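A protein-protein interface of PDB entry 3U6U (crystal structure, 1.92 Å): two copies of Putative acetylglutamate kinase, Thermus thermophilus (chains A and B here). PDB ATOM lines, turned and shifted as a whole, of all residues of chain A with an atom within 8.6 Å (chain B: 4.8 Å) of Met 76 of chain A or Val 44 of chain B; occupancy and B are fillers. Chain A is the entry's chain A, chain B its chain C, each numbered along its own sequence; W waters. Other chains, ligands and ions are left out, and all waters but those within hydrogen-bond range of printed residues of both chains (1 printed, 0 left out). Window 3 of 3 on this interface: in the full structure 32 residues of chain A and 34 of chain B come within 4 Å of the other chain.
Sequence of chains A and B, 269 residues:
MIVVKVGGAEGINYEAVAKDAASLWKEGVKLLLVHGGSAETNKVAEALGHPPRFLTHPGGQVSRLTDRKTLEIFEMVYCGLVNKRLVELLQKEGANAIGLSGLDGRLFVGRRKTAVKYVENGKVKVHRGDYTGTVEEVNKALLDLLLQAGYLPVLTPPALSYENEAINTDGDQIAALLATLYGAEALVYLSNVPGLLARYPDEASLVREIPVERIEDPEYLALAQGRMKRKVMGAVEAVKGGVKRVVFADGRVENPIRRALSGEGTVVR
The backbone carbonyl oxygen (O) of Glu 75 of chain A sits at hydrogen-bond distance from the backbone NH (N) of Gly 80 of chain A, at 3.2 Å.
O of Met 76 of chain A sits at hydrogen-bond distance from N of Leu 81 of chain A (3.0 Å).
The backbone carbonyl oxygen of Met 76 of chain B lies within hydrogen-bond range of the backbone NH of Leu 81 of chain B, at 2.9 Å.
Among the printed residues, pairs that only touch across the chains: Leu 48 of chain A with Leu 48 of chain B (3.4 Å), Met 76 of chain A with Met 76 of chain B (3.5 Å), Met 76 of chain A with Val 44 of chain B (3.6 Å), Glu 75 of chain A with Gly 80 of chain B (3.6 Å), Glu 72 of chain A with Leu 81 of chain B (3.7 Å), Met 76 of chain A with Val 77 of chain B (3.7 Å), Met 76 of chain A with Leu 81 of chain B (3.8 Å), Leu 81 of chain A with Met 76 of chain B (3.8 Å), Gly 80 of chain A with Gly 80 of chain B (3.8 Å), Ala 47 of chain A with Leu 48 of chain B (3.9 Å), Ala 47 of chain A with Ala 47 of chain B (3.9 Å) and Leu 48 of chain A with Ala 47 of chain B (3.9 Å).
Val 44 of chain A touches none of the printed residues of chain B.
Of the printed residues of chain B, Ala 47 of chain A touches Ala 47 (3.9 Å) and Leu 48 (3.9 Å).
Of chain B, only Val 44 (3.6 Å), Met 76 (3.5 Å), Val 77 (3.7 Å) and Leu 81 (3.8 Å) come within 4 Å of Met 76 of chain A.
Printed residues of chain B within 4 Å of Gly 80 of chain A: Gly 80 (3.8 Å).
Printed residues of chain B within 4 Å of Leu 81 of chain A: Met 76.
Of chain A, only Met 76 comes within 4 Å of Val 44 of chain B.
Ala 45 of chain B touches none of the printed residues of chain A.
Ile 73 of chain B touches none of the printed residues of chain A.
Of the printed residues of chain A, Val 77 of chain B touches Met 76.
Of the printed residues of chain A, Gly 80 of chain B touches Glu 75 and Gly 80.
Of the 14 printed residues of chain B, 7 touch a printed residue of chain A.
Printed residues of chain B that touch a printed residue of chain A: Val 44, Ala 47, Leu 48, Met 76, Val 77, Gly 80 and Leu 81.
Hydrophobic or aromatic side chains of chain B that line the printed part of chain A: Val 44, Ala 47, Leu 48, Met 76, Val 77 and Leu 81.
Printed residues of chain A that touch a printed residue of chain B: Ala 47, Leu 48, Glu 72, Glu 75, Met 76, Gly 80 and Leu 81.
Hydrophobic or aromatic side chains of chain A that line the printed part of chain B: Ala 47, Leu 48, Met 76 and Leu 81.
Among the printed residues, 12 pairs touch across the chains.
Among the printed residues, no Asp or Glu carboxylate lies within 4 Å of a Lys or Arg side-chain nitrogen of the other chain.
Ala 47 of chain A touches its own counterpart, Ala 47 of chain B.
Ala 47 of chain A touches Leu 48 of chain B, and with the chains exchanged Leu 48 of chain A touches Ala 47 of chain B.
Met 76 of chain A touches Val 44 of chain B, but with the chains exchanged Val 44 of chain A does not touch Met 76 of chain B (4.5 Å).
Gly 80 of chain A touches its own counterpart, Gly 80 of chain B.
Positions printed for both chains: 40, 41, 44, 45, 47, 48, 73, 76, 77, 80 and 81.
Water W1 lies within hydrogen-bond range of O of Leu 81 of chain B (2.7 Å) and OE1 of Glu 75 of chain A (2.7 Å).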
ATOM      1  N   GLY A  37     -35.569   5.591  -7.582  1.00  0.00           N
ATOM      2  CA  GLY A  37     -34.118   5.559  -7.536  1.00  0.00           C
ATOM      3  C   GLY A  37     -33.491   4.720  -8.638  1.00  0.00           C
ATOM      4  O   GLY A  37     -32.399   4.183  -8.465  1.00  0.00           O
ATOM      5  N   GLU A  40     -29.981   6.272 -10.066  1.00  0.00           N
ATOM      6  CA  GLU A  40     -28.902   6.114  -9.098  1.00  0.00           C
ATOM      7  C   GLU A  40     -28.577   4.649  -8.843  1.00  0.00           C
ATOM      8  O   GLU A  40     -27.438   4.309  -8.531  1.00  0.00           O
ATOM      9  CB  GLU A  40     -29.242   6.834  -7.784  1.00  0.00           C
ATOM     10  CG  GLU A  40     -29.357   8.352  -7.955  1.00  0.00           C
ATOM     11  CD  GLU A  40     -29.462   9.104  -6.636  1.00  0.00           C
ATOM     12  OE1 GLU A  40     -28.518   9.028  -5.825  1.00  0.00           O
ATOM     13  OE2 GLU A  40     -30.487   9.775  -6.415  1.00  0.00           O
ATOM     14  N   THR A  41     -29.573   3.779  -8.981  1.00  0.00           N
ATOM     15  CA  THR A  41     -29.346   2.353  -8.778  1.00  0.00           C
ATOM     16  C   THR A  41     -28.456   1.802  -9.900  1.00  0.00           C
ATOM     17  O   THR A  41     -27.535   1.026  -9.646  1.00  0.00           O
ATOM     18  CB  THR A  41     -30.680   1.575  -8.744  1.00  0.00           C
ATOM     19  OG1 THR A  41     -31.411   1.938  -7.567  1.00  0.00           O
ATOM     20  CG2 THR A  41     -30.427   0.071  -8.727  1.00  0.00           C
ATOM     21  N   VAL A  44     -24.778   2.787  -9.192  1.00  0.00           N
ATOM     22  CA  VAL A  44     -24.155   2.026  -8.115  1.00  0.00           C
ATOM     23  C   VAL A  44     -23.911   0.586  -8.548  1.00  0.00           C
ATOM     24  O   VAL A  44     -22.867   0.011  -8.242  1.00  0.00           O
ATOM     25  CB  VAL A  44     -25.030   2.024  -6.837  1.00  0.00           C
ATOM     26  CG1 VAL A  44     -24.410   1.118  -5.783  1.00  0.00           C
ATOM     27  CG2 VAL A  44     -25.160   3.440  -6.300  1.00  0.00           C
ATOM     28  N   ALA A  45     -24.878   0.005  -9.252  1.00  0.00           N
ATOM     29  CA  ALA A  45     -24.757  -1.370  -9.732  1.00  0.00           C
ATOM     30  C   ALA A  45     -23.533  -1.459 -10.641  1.00  0.00           C
ATOM     31  O   ALA A  45     -22.753  -2.413 -10.573  1.00  0.00           O
ATOM     32  CB  ALA A  45     -26.013  -1.770 -10.501  1.00  0.00           C
ATOM     33  N   ALA A  47     -20.869   0.580 -10.667  1.00  0.00           N
ATOM     34  CA  ALA A  47     -19.689   0.730  -9.823  1.00  0.00           C
ATOM     35  C   ALA A  47     -19.370  -0.509  -8.991  1.00  0.00           C
ATOM     36  O   ALA A  47     -18.221  -0.718  -8.600  1.00  0.00           O
ATOM     37  CB  ALA A  47     -19.861   1.935  -8.910  1.00  0.00           C
ATOM     38  N   LEU A  48     -20.382  -1.327  -8.715  1.00  0.00           N
ATOM     39  CA  LEU A  48     -20.176  -2.531  -7.918  1.00  0.00           C
ATOM     40  C   LEU A  48     -19.841  -3.747  -8.771  1.00  0.00           C
ATOM     41  O   LEU A  48     -19.690  -4.856  -8.255  1.00  0.00           O
ATOM     42  CB  LEU A  48     -21.414  -2.818  -7.065  1.00  0.00           C
ATOM     43  CG  LEU A  48     -21.669  -1.824  -5.927  1.00  0.00           C
ATOM     44  CD1 LEU A  48     -22.982  -2.155  -5.240  1.00  0.00           C
ATOM     45  CD2 LEU A  48     -20.515  -1.876  -4.937  1.00  0.00           C
ATOM     46  N   LYS A  69     -28.861 -10.530  -5.975  1.00  0.00           N
ATOM     47  CA  LYS A  69     -27.843  -9.499  -5.847  1.00  0.00           C
ATOM     48  C   LYS A  69     -28.352  -8.132  -6.297  1.00  0.00           C
ATOM     49  O   LYS A  69     -28.107  -7.125  -5.634  1.00  0.00           O
ATOM     50  CB  LYS A  69     -26.593  -9.902  -6.637  1.00  0.00           C
ATOM     51  CG  LYS A  69     -25.627  -8.766  -6.937  1.00  0.00           C
ATOM     52  CD  LYS A  69     -25.859  -8.207  -8.336  1.00  0.00           C
ATOM     53  CE  LYS A  69     -25.750  -9.312  -9.390  1.00  0.00           C
ATOM     54  NZ  LYS A  69     -25.321  -8.790 -10.718  1.00  0.00           N
ATOM     55  N   THR A  70     -29.065  -8.098  -7.418  1.00  0.00           N
ATOM     56  CA  THR A  70     -29.604  -6.844  -7.929  1.00  0.00           C
ATOM     57  C   THR A  70     -30.606  -6.255  -6.937  1.00  0.00           C
ATOM     58  O   THR A  70     -30.657  -5.039  -6.739  1.00  0.00           O
ATOM     59  CB  THR A  70     -30.299  -7.049  -9.299  1.00  0.00           C
ATOM     60  OG1 THR A  70     -29.322  -7.429 -10.279  1.00  0.00           O
ATOM     61  CG2 THR A  70     -30.990  -5.767  -9.755  1.00  0.00           C
ATOM     62  N   LEU A  71     -31.400  -7.121  -6.315  1.00  0.00           N
ATOM     63  CA  LEU A  71     -32.395  -6.677  -5.349  1.00  0.00           C
ATOM     64  C   LEU A  71     -31.702  -6.033  -4.146  1.00  0.00           C
ATOM     65  O   LEU A  71     -32.207  -5.064  -3.580  1.00  0.00           O
ATOM     66  CB  LEU A  71     -33.260  -7.856  -4.894  1.00  0.00           C
ATOM     67  CG  LEU A  71     -34.456  -7.515  -4.000  1.00  0.00           C
ATOM     68  CD1 LEU A  71     -35.341  -6.484  -4.689  1.00  0.00           C
ATOM     69  CD2 LEU A  71     -35.245  -8.779  -3.700  1.00  0.00           C
ATOM     70  N   GLU A  72     -30.543  -6.570  -3.771  1.00  0.00           N
ATOM     71  CA  GLU A  72     -29.784  -6.029  -2.651  1.00  0.00           C
ATOM     72  C   GLU A  72     -29.285  -4.626  -2.984  1.00  0.00           C
ATOM     73  O   GLU A  72     -29.318  -3.730  -2.138  1.00  0.00           O
ATOM     74  CB  GLU A  72     -28.589  -6.923  -2.318  1.00  0.00           C
ATOM     75  CG  GLU A  72     -28.957  -8.348  -1.970  1.00  0.00           C
ATOM     76  CD  GLU A  72     -27.784  -9.129  -1.416  1.00  0.00           C
ATOM     77  OE1 GLU A  72     -26.670  -9.007  -1.971  1.00  0.00           O
ATOM     78  OE2 GLU A  72     -27.974  -9.871  -0.432  1.00  0.00           O
ATOM     79  N   ILE A  73     -28.813  -4.440  -4.216  1.00  0.00           N
ATOM     80  CA  ILE A  73     -28.320  -3.136  -4.641  1.00  0.00           C
ATOM     81  C   ILE A  73     -29.503  -2.173  -4.717  1.00  0.00           C
ATOM     82  O   ILE A  73     -29.399  -1.001  -4.343  1.00  0.00           O
ATOM     83  CB  ILE A  73     -27.619  -3.224  -6.018  1.00  0.00           C
ATOM     84  CG1 ILE A  73     -26.406  -4.156  -5.911  1.00  0.00           C
ATOM     85  CG2 ILE A  73     -27.183  -1.827  -6.475  1.00  0.00           C
ATOM     86  CD1 ILE A  73     -25.671  -4.386  -7.223  1.00  0.00           C
ATOM     87  N   PHE A  74     -30.626  -2.691  -5.200  1.00  0.00           N
ATOM     88  CA  PHE A  74     -31.867  -1.934  -5.319  1.00  0.00           C
ATOM     89  C   PHE A  74     -32.248  -1.404  -3.927  1.00  0.00           C
ATOM     90  O   PHE A  74     -32.586  -0.230  -3.765  1.00  0.00           O
ATOM     91  CB  PHE A  74     -32.966  -2.867  -5.839  1.00  0.00           C
ATOM     92  CG  PHE A  74     -34.297  -2.203  -6.057  1.00  0.00           C
ATOM     93  CD1 PHE A  74     -34.704  -1.837  -7.334  1.00  0.00           C
ATOM     94  CD2 PHE A  74     -35.161  -1.971  -4.987  1.00  0.00           C
ATOM     95  CE1 PHE A  74     -35.952  -1.252  -7.551  1.00  0.00           C
ATOM     96  CE2 PHE A  74     -36.408  -1.388  -5.190  1.00  0.00           C
ATOM     97  CZ  PHE A  74     -36.807  -1.026  -6.474  1.00  0.00           C
ATOM     98  N   GLU A  75     -32.197  -2.282  -2.926  1.00  0.00           N
ATOM     99  CA  GLU A  75     -32.540  -1.888  -1.562  1.00  0.00           C
ATOM    100  C   GLU A  75     -31.547  -0.864  -1.019  1.00  0.00           C
ATOM    101  O   GLU A  75     -31.944   0.131  -0.416  1.00  0.00           O
ATOM    102  CB  GLU A  75     -32.605  -3.118  -0.652  1.00  0.00           C
ATOM    103  CG  GLU A  75     -33.747  -4.062  -1.012  1.00  0.00           C
ATOM    104  CD  GLU A  75     -33.806  -5.296  -0.132  1.00  0.00           C
ATOM    105  OE1 GLU A  75     -32.739  -5.782   0.287  1.00  0.00           O
ATOM    106  OE2 GLU A  75     -34.923  -5.794   0.125  1.00  0.00           O
ATOM    107  N   MET A  76     -30.257  -1.100  -1.244  1.00  0.00           N
ATOM    108  CA  MET A  76     -29.237  -0.165  -0.781  1.00  0.00           C
ATOM    109  C   MET A  76     -29.533   1.259  -1.246  1.00  0.00           C
ATOM    110  O   MET A  76     -29.495   2.208  -0.453  1.00  0.00           O
ATOM    111  CB  MET A  76     -27.848  -0.585  -1.288  1.00  0.00           C
ATOM    112  CG  MET A  76     -27.216  -1.737  -0.513  1.00  0.00           C
ATOM    113  SD  MET A  76     -25.570  -2.226  -1.137  1.00  0.00           S
ATOM    114  CE  MET A  76     -24.602  -1.021  -0.438  1.00  0.00           C
ATOM    115  N   VAL A  77     -29.853   1.402  -2.527  1.00  0.00           N
ATOM    116  CA  VAL A  77     -30.119   2.715  -3.103  1.00  0.00           C
ATOM    117  C   VAL A  77     -31.510   3.282  -2.833  1.00  0.00           C
ATOM    118  O   VAL A  77     -31.631   4.420  -2.380  1.00  0.00           O
ATOM    119  CB  VAL A  77     -29.860   2.703  -4.638  1.00  0.00           C
ATOM    120  CG1 VAL A  77     -30.190   4.065  -5.241  1.00  0.00           C
ATOM    121  CG2 VAL A  77     -28.401   2.349  -4.907  1.00  0.00           C
ATOM    122  N   TYR A  78     -32.557   2.509  -3.120  1.00  0.00           N
ATOM    123  CA  TYR A  78     -33.921   2.981  -2.887  1.00  0.00           C
ATOM    124  C   TYR A  78     -34.235   3.181  -1.408  1.00  0.00           C
ATOM    125  O   TYR A  78     -34.654   4.261  -0.995  1.00  0.00           O
ATOM    126  CB  TYR A  78     -34.956   1.996  -3.446  1.00  0.00           C
ATOM    127  CG  TYR A  78     -35.241   2.113  -4.928  1.00  0.00           C
ATOM    128  CD1 TYR A  78     -34.282   1.754  -5.874  1.00  0.00           C
ATOM    129  CD2 TYR A  78     -36.494   2.529  -5.383  1.00  0.00           C
ATOM    130  CE1 TYR A  78     -34.561   1.795  -7.235  1.00  0.00           C
ATOM    131  CE2 TYR A  78     -36.785   2.578  -6.746  1.00  0.00           C
ATOM    132  CZ  TYR A  78     -35.811   2.205  -7.664  1.00  0.00           C
ATOM    133  OH  TYR A  78     -36.088   2.220  -9.009  1.00  0.00           O
ATOM    134  N   CYS A  79     -34.025   2.127  -0.625  1.00  0.00           N
ATOM    135  CA  CYS A  79     -34.332   2.131   0.802  1.00  0.00           C
ATOM    136  C   CYS A  79     -33.317   2.821   1.700  1.00  0.00           C
ATOM    137  O   CYS A  79     -33.672   3.323   2.770  1.00  0.00           O
ATOM    138  CB  CYS A  79     -34.529   0.689   1.277  1.00  0.00           C
ATOM    139  SG  CYS A  79     -35.684  -0.247   0.247  1.00  0.00           S
ATOM    140  N   GLY A  80     -32.056   2.831   1.279  1.00  0.00           N
ATOM    141  CA  GLY A  80     -31.025   3.468   2.079  1.00  0.00           C
ATOM    142  C   GLY A  80     -30.668   4.872   1.624  1.00  0.00           C
ATOM    143  O   GLY A  80     -30.976   5.859   2.298  1.00  0.00           O
ATOM    144  N   LEU A  81     -30.019   4.962   0.468  1.00  0.00           N
ATOM    145  CA  LEU A  81     -29.577   6.243  -0.074  1.00  0.00           C
ATOM    146  C   LEU A  81     -30.676   7.277  -0.300  1.00  0.00           C
ATOM    147  O   LEU A  81     -30.681   8.335   0.326  1.00  0.00           O
ATOM    148  CB  LEU A  81     -28.830   6.017  -1.395  1.00  0.00           C
ATOM    149  CG  LEU A  81     -28.219   7.271  -2.035  1.00  0.00           C
ATOM    150  CD1 LEU A  81     -27.042   7.749  -1.194  1.00  0.00           C
ATOM    151  CD2 LEU A  81     -27.762   6.959  -3.454  1.00  0.00           C
ATOM    152  N   VAL A  82     -31.607   6.971  -1.196  1.00  0.00           N
ATOM    153  CA  VAL A  82     -32.670   7.907  -1.521  1.00  0.00           C
ATOM    154  C   VAL A  82     -33.704   8.136  -0.421  1.00  0.00           C
ATOM    155  O   VAL A  82     -34.059   9.276  -0.135  1.00  0.00           O
ATOM    156  CB  VAL A  82     -33.396   7.481  -2.817  1.00  0.00           C
ATOM    157  CG1 VAL A  82     -34.410   8.539  -3.217  1.00  0.00           C
ATOM    158  CG2 VAL A  82     -32.370   7.269  -3.943  1.00  0.00           C
ATOM    159  N   ASN A  83     -34.187   7.063   0.200  1.00  0.00           N
ATOM    160  CA  ASN A  83     -35.194   7.211   1.246  1.00  0.00           C
ATOM    161  C   ASN A  83     -34.676   8.073   2.405  1.00  0.00           C
ATOM    162  O   ASN A  83     -35.339   9.019   2.824  1.00  0.00           O
ATOM    163  CB  ASN A  83     -35.634   5.831   1.755  1.00  0.00           C
ATOM    164  CG  ASN A  83     -36.856   5.899   2.664  1.00  0.00           C
ATOM    165  OD1 ASN A  83     -36.757   5.691   3.876  1.00  0.00           O
ATOM    166  ND2 ASN A  83     -38.015   6.185   2.079  1.00  0.00           N
ATOM    167  N   LYS A  84     -33.484   7.764   2.905  1.00  0.00           N
ATOM    168  CA  LYS A  84     -32.936   8.522   4.023  1.00  0.00           C
ATOM    169  C   LYS A  84     -32.499   9.931   3.635  1.00  0.00           C
ATOM    170  O   LYS A  84     -32.514  10.839   4.466  1.00  0.00           O
ATOM    171  CB  LYS A  84     -31.782   7.750   4.671  1.00  0.00           C
ATOM    172  CG  LYS A  84     -32.178   6.329   5.088  1.00  0.00           C
ATOM    173  CD  LYS A  84     -33.564   6.284   5.731  1.00  0.00           C
ATOM    174  CE  LYS A  84     -34.028   4.839   5.965  1.00  0.00           C
ATOM    175  NZ  LYS A  84     -35.457   4.768   6.399  1.00  0.00           N
ATOM    176  N   PRO A 157     -40.451   1.187  -2.936  1.00  0.00           N
ATOM    177  CA  PRO A 157     -40.443  -0.266  -3.121  1.00  0.00           C
ATOM    178  C   PRO A 157     -39.134  -0.686  -2.445  1.00  0.00           C
ATOM    179  O   PRO A 157     -38.349   0.174  -2.054  1.00  0.00           O
ATOM    180  CB  PRO A 157     -40.409  -0.431  -4.646  1.00  0.00           C
ATOM    181  CG  PRO A 157     -39.831   0.883  -5.142  1.00  0.00           C
ATOM    182  CD  PRO A 157     -40.495   1.886  -4.233  1.00  0.00           C
ATOM    183  N   PRO A 158     -38.844  -1.992  -2.356  1.00  0.00           N
ATOM    184  CA  PRO A 158     -39.614  -3.147  -2.816  1.00  0.00           C
ATOM    185  C   PRO A 158     -40.882  -3.442  -2.038  1.00  0.00           C
ATOM    186  O   PRO A 158     -41.162  -2.830  -1.002  1.00  0.00           O
ATOM    187  CB  PRO A 158     -38.607  -4.284  -2.710  1.00  0.00           C
ATOM    188  CG  PRO A 158     -37.859  -3.928  -1.477  1.00  0.00           C
ATOM    189  CD  PRO A 158     -37.634  -2.430  -1.635  1.00  0.00           C
ATOM    190  N   GLU B  40     -19.918  -5.048   6.827  1.00  0.00           N
ATOM    191  CA  GLU B  40     -20.439  -5.000   5.467  1.00  0.00           C
ATOM    192  C   GLU B  40     -20.291  -3.614   4.856  1.00  0.00           C
ATOM    193  O   GLU B  40     -20.176  -3.478   3.637  1.00  0.00           O
ATOM    194  CB  GLU B  40     -21.903  -5.446   5.431  1.00  0.00           C
ATOM    195  CG  GLU B  40     -22.073  -6.927   5.748  1.00  0.00           C
ATOM    196  CD  GLU B  40     -23.501  -7.409   5.578  1.00  0.00           C
ATOM    197  OE1 GLU B  40     -24.006  -7.391   4.437  1.00  0.00           O
ATOM    198  OE2 GLU B  40     -24.116  -7.805   6.588  1.00  0.00           O
ATOM    199  N   THR B  41     -20.294  -2.588   5.701  1.00  0.00           N
ATOM    200  CA  THR B  41     -20.135  -1.220   5.224  1.00  0.00           C
ATOM    201  C   THR B  41     -18.694  -1.028   4.737  1.00  0.00           C
ATOM    202  O   THR B  41     -18.459  -0.427   3.687  1.00  0.00           O
ATOM    203  CB  THR B  41     -20.457  -0.201   6.344  1.00  0.00           C
ATOM    204  OG1 THR B  41     -21.862  -0.244   6.632  1.00  0.00           O
ATOM    205  CG2 THR B  41     -20.083   1.210   5.918  1.00  0.00           C
ATOM    206  N   ASN B  42     -17.736  -1.550   5.499  1.00  0.00           N
ATOM    207  CA  ASN B  42     -16.327  -1.438   5.127  1.00  0.00           C
ATOM    208  C   ASN B  42     -16.095  -2.065   3.763  1.00  0.00           C
ATOM    209  O   ASN B  42     -15.429  -1.485   2.911  1.00  0.00           O
ATOM    210  CB  ASN B  42     -15.433  -2.136   6.152  1.00  0.00           C
ATOM    211  CG  ASN B  42     -15.465  -1.467   7.502  1.00  0.00           C
ATOM    212  OD1 ASN B  42     -15.716  -0.264   7.605  1.00  0.00           O
ATOM    213  ND2 ASN B  42     -15.192  -2.237   8.551  1.00  0.00           N
ATOM    214  N   LYS B  43     -16.656  -3.255   3.565  1.00  0.00           N
ATOM    215  CA  LYS B  43     -16.514  -3.971   2.305  1.00  0.00           C
ATOM    216  C   LYS B  43     -17.098  -3.192   1.133  1.00  0.00           C
ATOM    217  O   LYS B  43     -16.458  -3.056   0.088  1.00  0.00           O
ATOM    218  CB  LYS B  43     -17.188  -5.341   2.399  1.00  0.00           C
ATOM    219  CG  LYS B  43     -17.124  -6.149   1.111  1.00  0.00           C
ATOM    220  CD  LYS B  43     -17.746  -7.524   1.289  1.00  0.00           C
ATOM    221  CE  LYS B  43     -17.659  -8.339   0.008  1.00  0.00           C
ATOM    222  NZ  LYS B  43     -18.214  -9.710   0.186  1.00  0.00           N
ATOM    223  N   VAL B  44     -18.315  -2.685   1.304  1.00  0.00           N
ATOM    224  CA  VAL B  44     -18.968  -1.919   0.247  1.00  0.00           C
ATOM    225  C   VAL B  44     -18.232  -0.612  -0.036  1.00  0.00           C
ATOM    226  O   VAL B  44     -18.166  -0.165  -1.182  1.00  0.00           O
ATOM    227  CB  VAL B  44     -20.434  -1.596   0.609  1.00  0.00           C
ATOM    228  CG1 VAL B  44     -21.014  -0.614  -0.398  1.00  0.00           C
ATOM    229  CG2 VAL B  44     -21.257  -2.877   0.622  1.00  0.00           C
ATOM    230  N   ALA B  45     -17.684  -0.002   1.010  1.00  0.00           N
ATOM    231  CA  ALA B  45     -16.952   1.250   0.861  1.00  0.00           C
ATOM    232  C   ALA B  45     -15.714   1.022  -0.010  1.00  0.00           C
ATOM    233  O   ALA B  45     -15.392   1.840  -0.872  1.00  0.00           O
ATOM    234  CB  ALA B  45     -16.548   1.787   2.233  1.00  0.00           C
ATOM    235  N   GLU B  46     -15.027  -0.092   0.227  1.00  0.00           N
ATOM    236  CA  GLU B  46     -13.837  -0.446  -0.542  1.00  0.00           C
ATOM    237  C   GLU B  46     -14.230  -0.670  -1.996  1.00  0.00           C
ATOM    238  O   GLU B  46     -13.592  -0.151  -2.911  1.00  0.00           O
ATOM    239  CB  GLU B  46     -13.207  -1.727   0.017  1.00  0.00           C
ATOM    240  CG  GLU B  46     -12.601  -1.572   1.402  1.00  0.00           C
ATOM    241  CD  GLU B  46     -11.219  -0.947   1.372  1.00  0.00           C
ATOM    242  OE1 GLU B  46     -10.983  -0.059   0.524  1.00  0.00           O
ATOM    243  OE2 GLU B  46     -10.373  -1.335   2.206  1.00  0.00           O
ATOM    244  N   ALA B  47     -15.291  -1.443  -2.199  1.00  0.00           N
ATOM    245  CA  ALA B  47     -15.775  -1.748  -3.539  1.00  0.00           C
ATOM    246  C   ALA B  47     -16.116  -0.491  -4.333  1.00  0.00           C
ATOM    247  O   ALA B  47     -15.839  -0.417  -5.530  1.00  0.00           O
ATOM    248  CB  ALA B  47     -16.993  -2.659  -3.456  1.00  0.00           C
ATOM    249  N   LEU B  48     -16.714   0.494  -3.669  1.00  0.00           N
ATOM    250  CA  LEU B  48     -17.094   1.737  -4.334  1.00  0.00           C
ATOM    251  C   LEU B  48     -15.934   2.717  -4.482  1.00  0.00           C
ATOM    252  O   LEU B  48     -16.129   3.861  -4.891  1.00  0.00           O
ATOM    253  CB  LEU B  48     -18.243   2.411  -3.583  1.00  0.00           C
ATOM    254  CG  LEU B  48     -19.579   1.665  -3.620  1.00  0.00           C
ATOM    255  CD1 LEU B  48     -20.613   2.420  -2.797  1.00  0.00           C
ATOM    256  CD2 LEU B  48     -20.041   1.519  -5.062  1.00  0.00           C
ATOM    257  N   ILE B  73     -22.797   5.920   2.098  1.00  0.00           N
ATOM    258  CA  ILE B  73     -22.496   4.496   1.958  1.00  0.00           C
ATOM    259  C   ILE B  73     -22.997   3.796   3.216  1.00  0.00           C
ATOM    260  O   ILE B  73     -23.529   2.684   3.163  1.00  0.00           O
ATOM    261  CB  ILE B  73     -20.971   4.250   1.793  1.00  0.00           C
ATOM    262  CG1 ILE B  73     -20.494   4.876   0.477  1.00  0.00           C
ATOM    263  CG2 ILE B  73     -20.667   2.753   1.807  1.00  0.00           C
ATOM    264  CD1 ILE B  73     -19.008   4.740   0.223  1.00  0.00           C
ATOM    265  N   MET B  76     -26.653   3.316   2.885  1.00  0.00           N
ATOM    266  CA  MET B  76     -26.970   2.270   1.921  1.00  0.00           C
ATOM    267  C   MET B  76     -26.907   0.895   2.580  1.00  0.00           C
ATOM    268  O   MET B  76     -27.818   0.085   2.431  1.00  0.00           O
ATOM    269  CB  MET B  76     -25.995   2.308   0.726  1.00  0.00           C
ATOM    270  CG  MET B  76     -26.207   3.481  -0.232  1.00  0.00           C
ATOM    271  SD  MET B  76     -25.218   3.349  -1.784  1.00  0.00           S
ATOM    272  CE  MET B  76     -23.700   3.743  -1.206  1.00  0.00           C
ATOM    273  N   VAL B  77     -25.836   0.643   3.322  1.00  0.00           N
ATOM    274  CA  VAL B  77     -25.654  -0.645   3.973  1.00  0.00           C
ATOM    275  C   VAL B  77     -26.519  -0.843   5.218  1.00  0.00           C
ATOM    276  O   VAL B  77     -27.253  -1.827   5.312  1.00  0.00           O
ATOM    277  CB  VAL B  77     -24.165  -0.871   4.341  1.00  0.00           C
ATOM    278  CG1 VAL B  77     -23.997  -2.204   5.057  1.00  0.00           C
ATOM    279  CG2 VAL B  77     -23.308  -0.856   3.071  1.00  0.00           C
ATOM    280  N   GLY B  80     -30.367   0.320   4.159  1.00  0.00           N
ATOM    281  CA  GLY B  80     -30.898  -0.389   3.012  1.00  0.00           C
ATOM    282  C   GLY B  80     -30.664  -1.889   3.077  1.00  0.00           C
ATOM    283  O   GLY B  80     -31.587  -2.662   3.312  1.00  0.00           O
ATOM    284  N   LEU B  81     -29.414  -2.297   2.892  1.00  0.00           N
ATOM    285  CA  LEU B  81     -29.053  -3.706   2.889  1.00  0.00           C
ATOM    286  C   LEU B  81     -29.424  -4.498   4.141  1.00  0.00           C
ATOM    287  O   LEU B  81     -30.255  -5.404   4.089  1.00  0.00           O
ATOM    288  CB  LEU B  81     -27.548  -3.857   2.642  1.00  0.00           C
ATOM    289  CG  LEU B  81     -27.017  -5.276   2.407  1.00  0.00           C
ATOM    290  CD1 LEU B  81     -27.478  -5.782   1.043  1.00  0.00           C
ATOM    291  CD2 LEU B  81     -25.496  -5.268   2.471  1.00  0.00           C
HETATM  292  O   HOH W   1     -30.848  -6.855   1.908  1.00  0.00           O
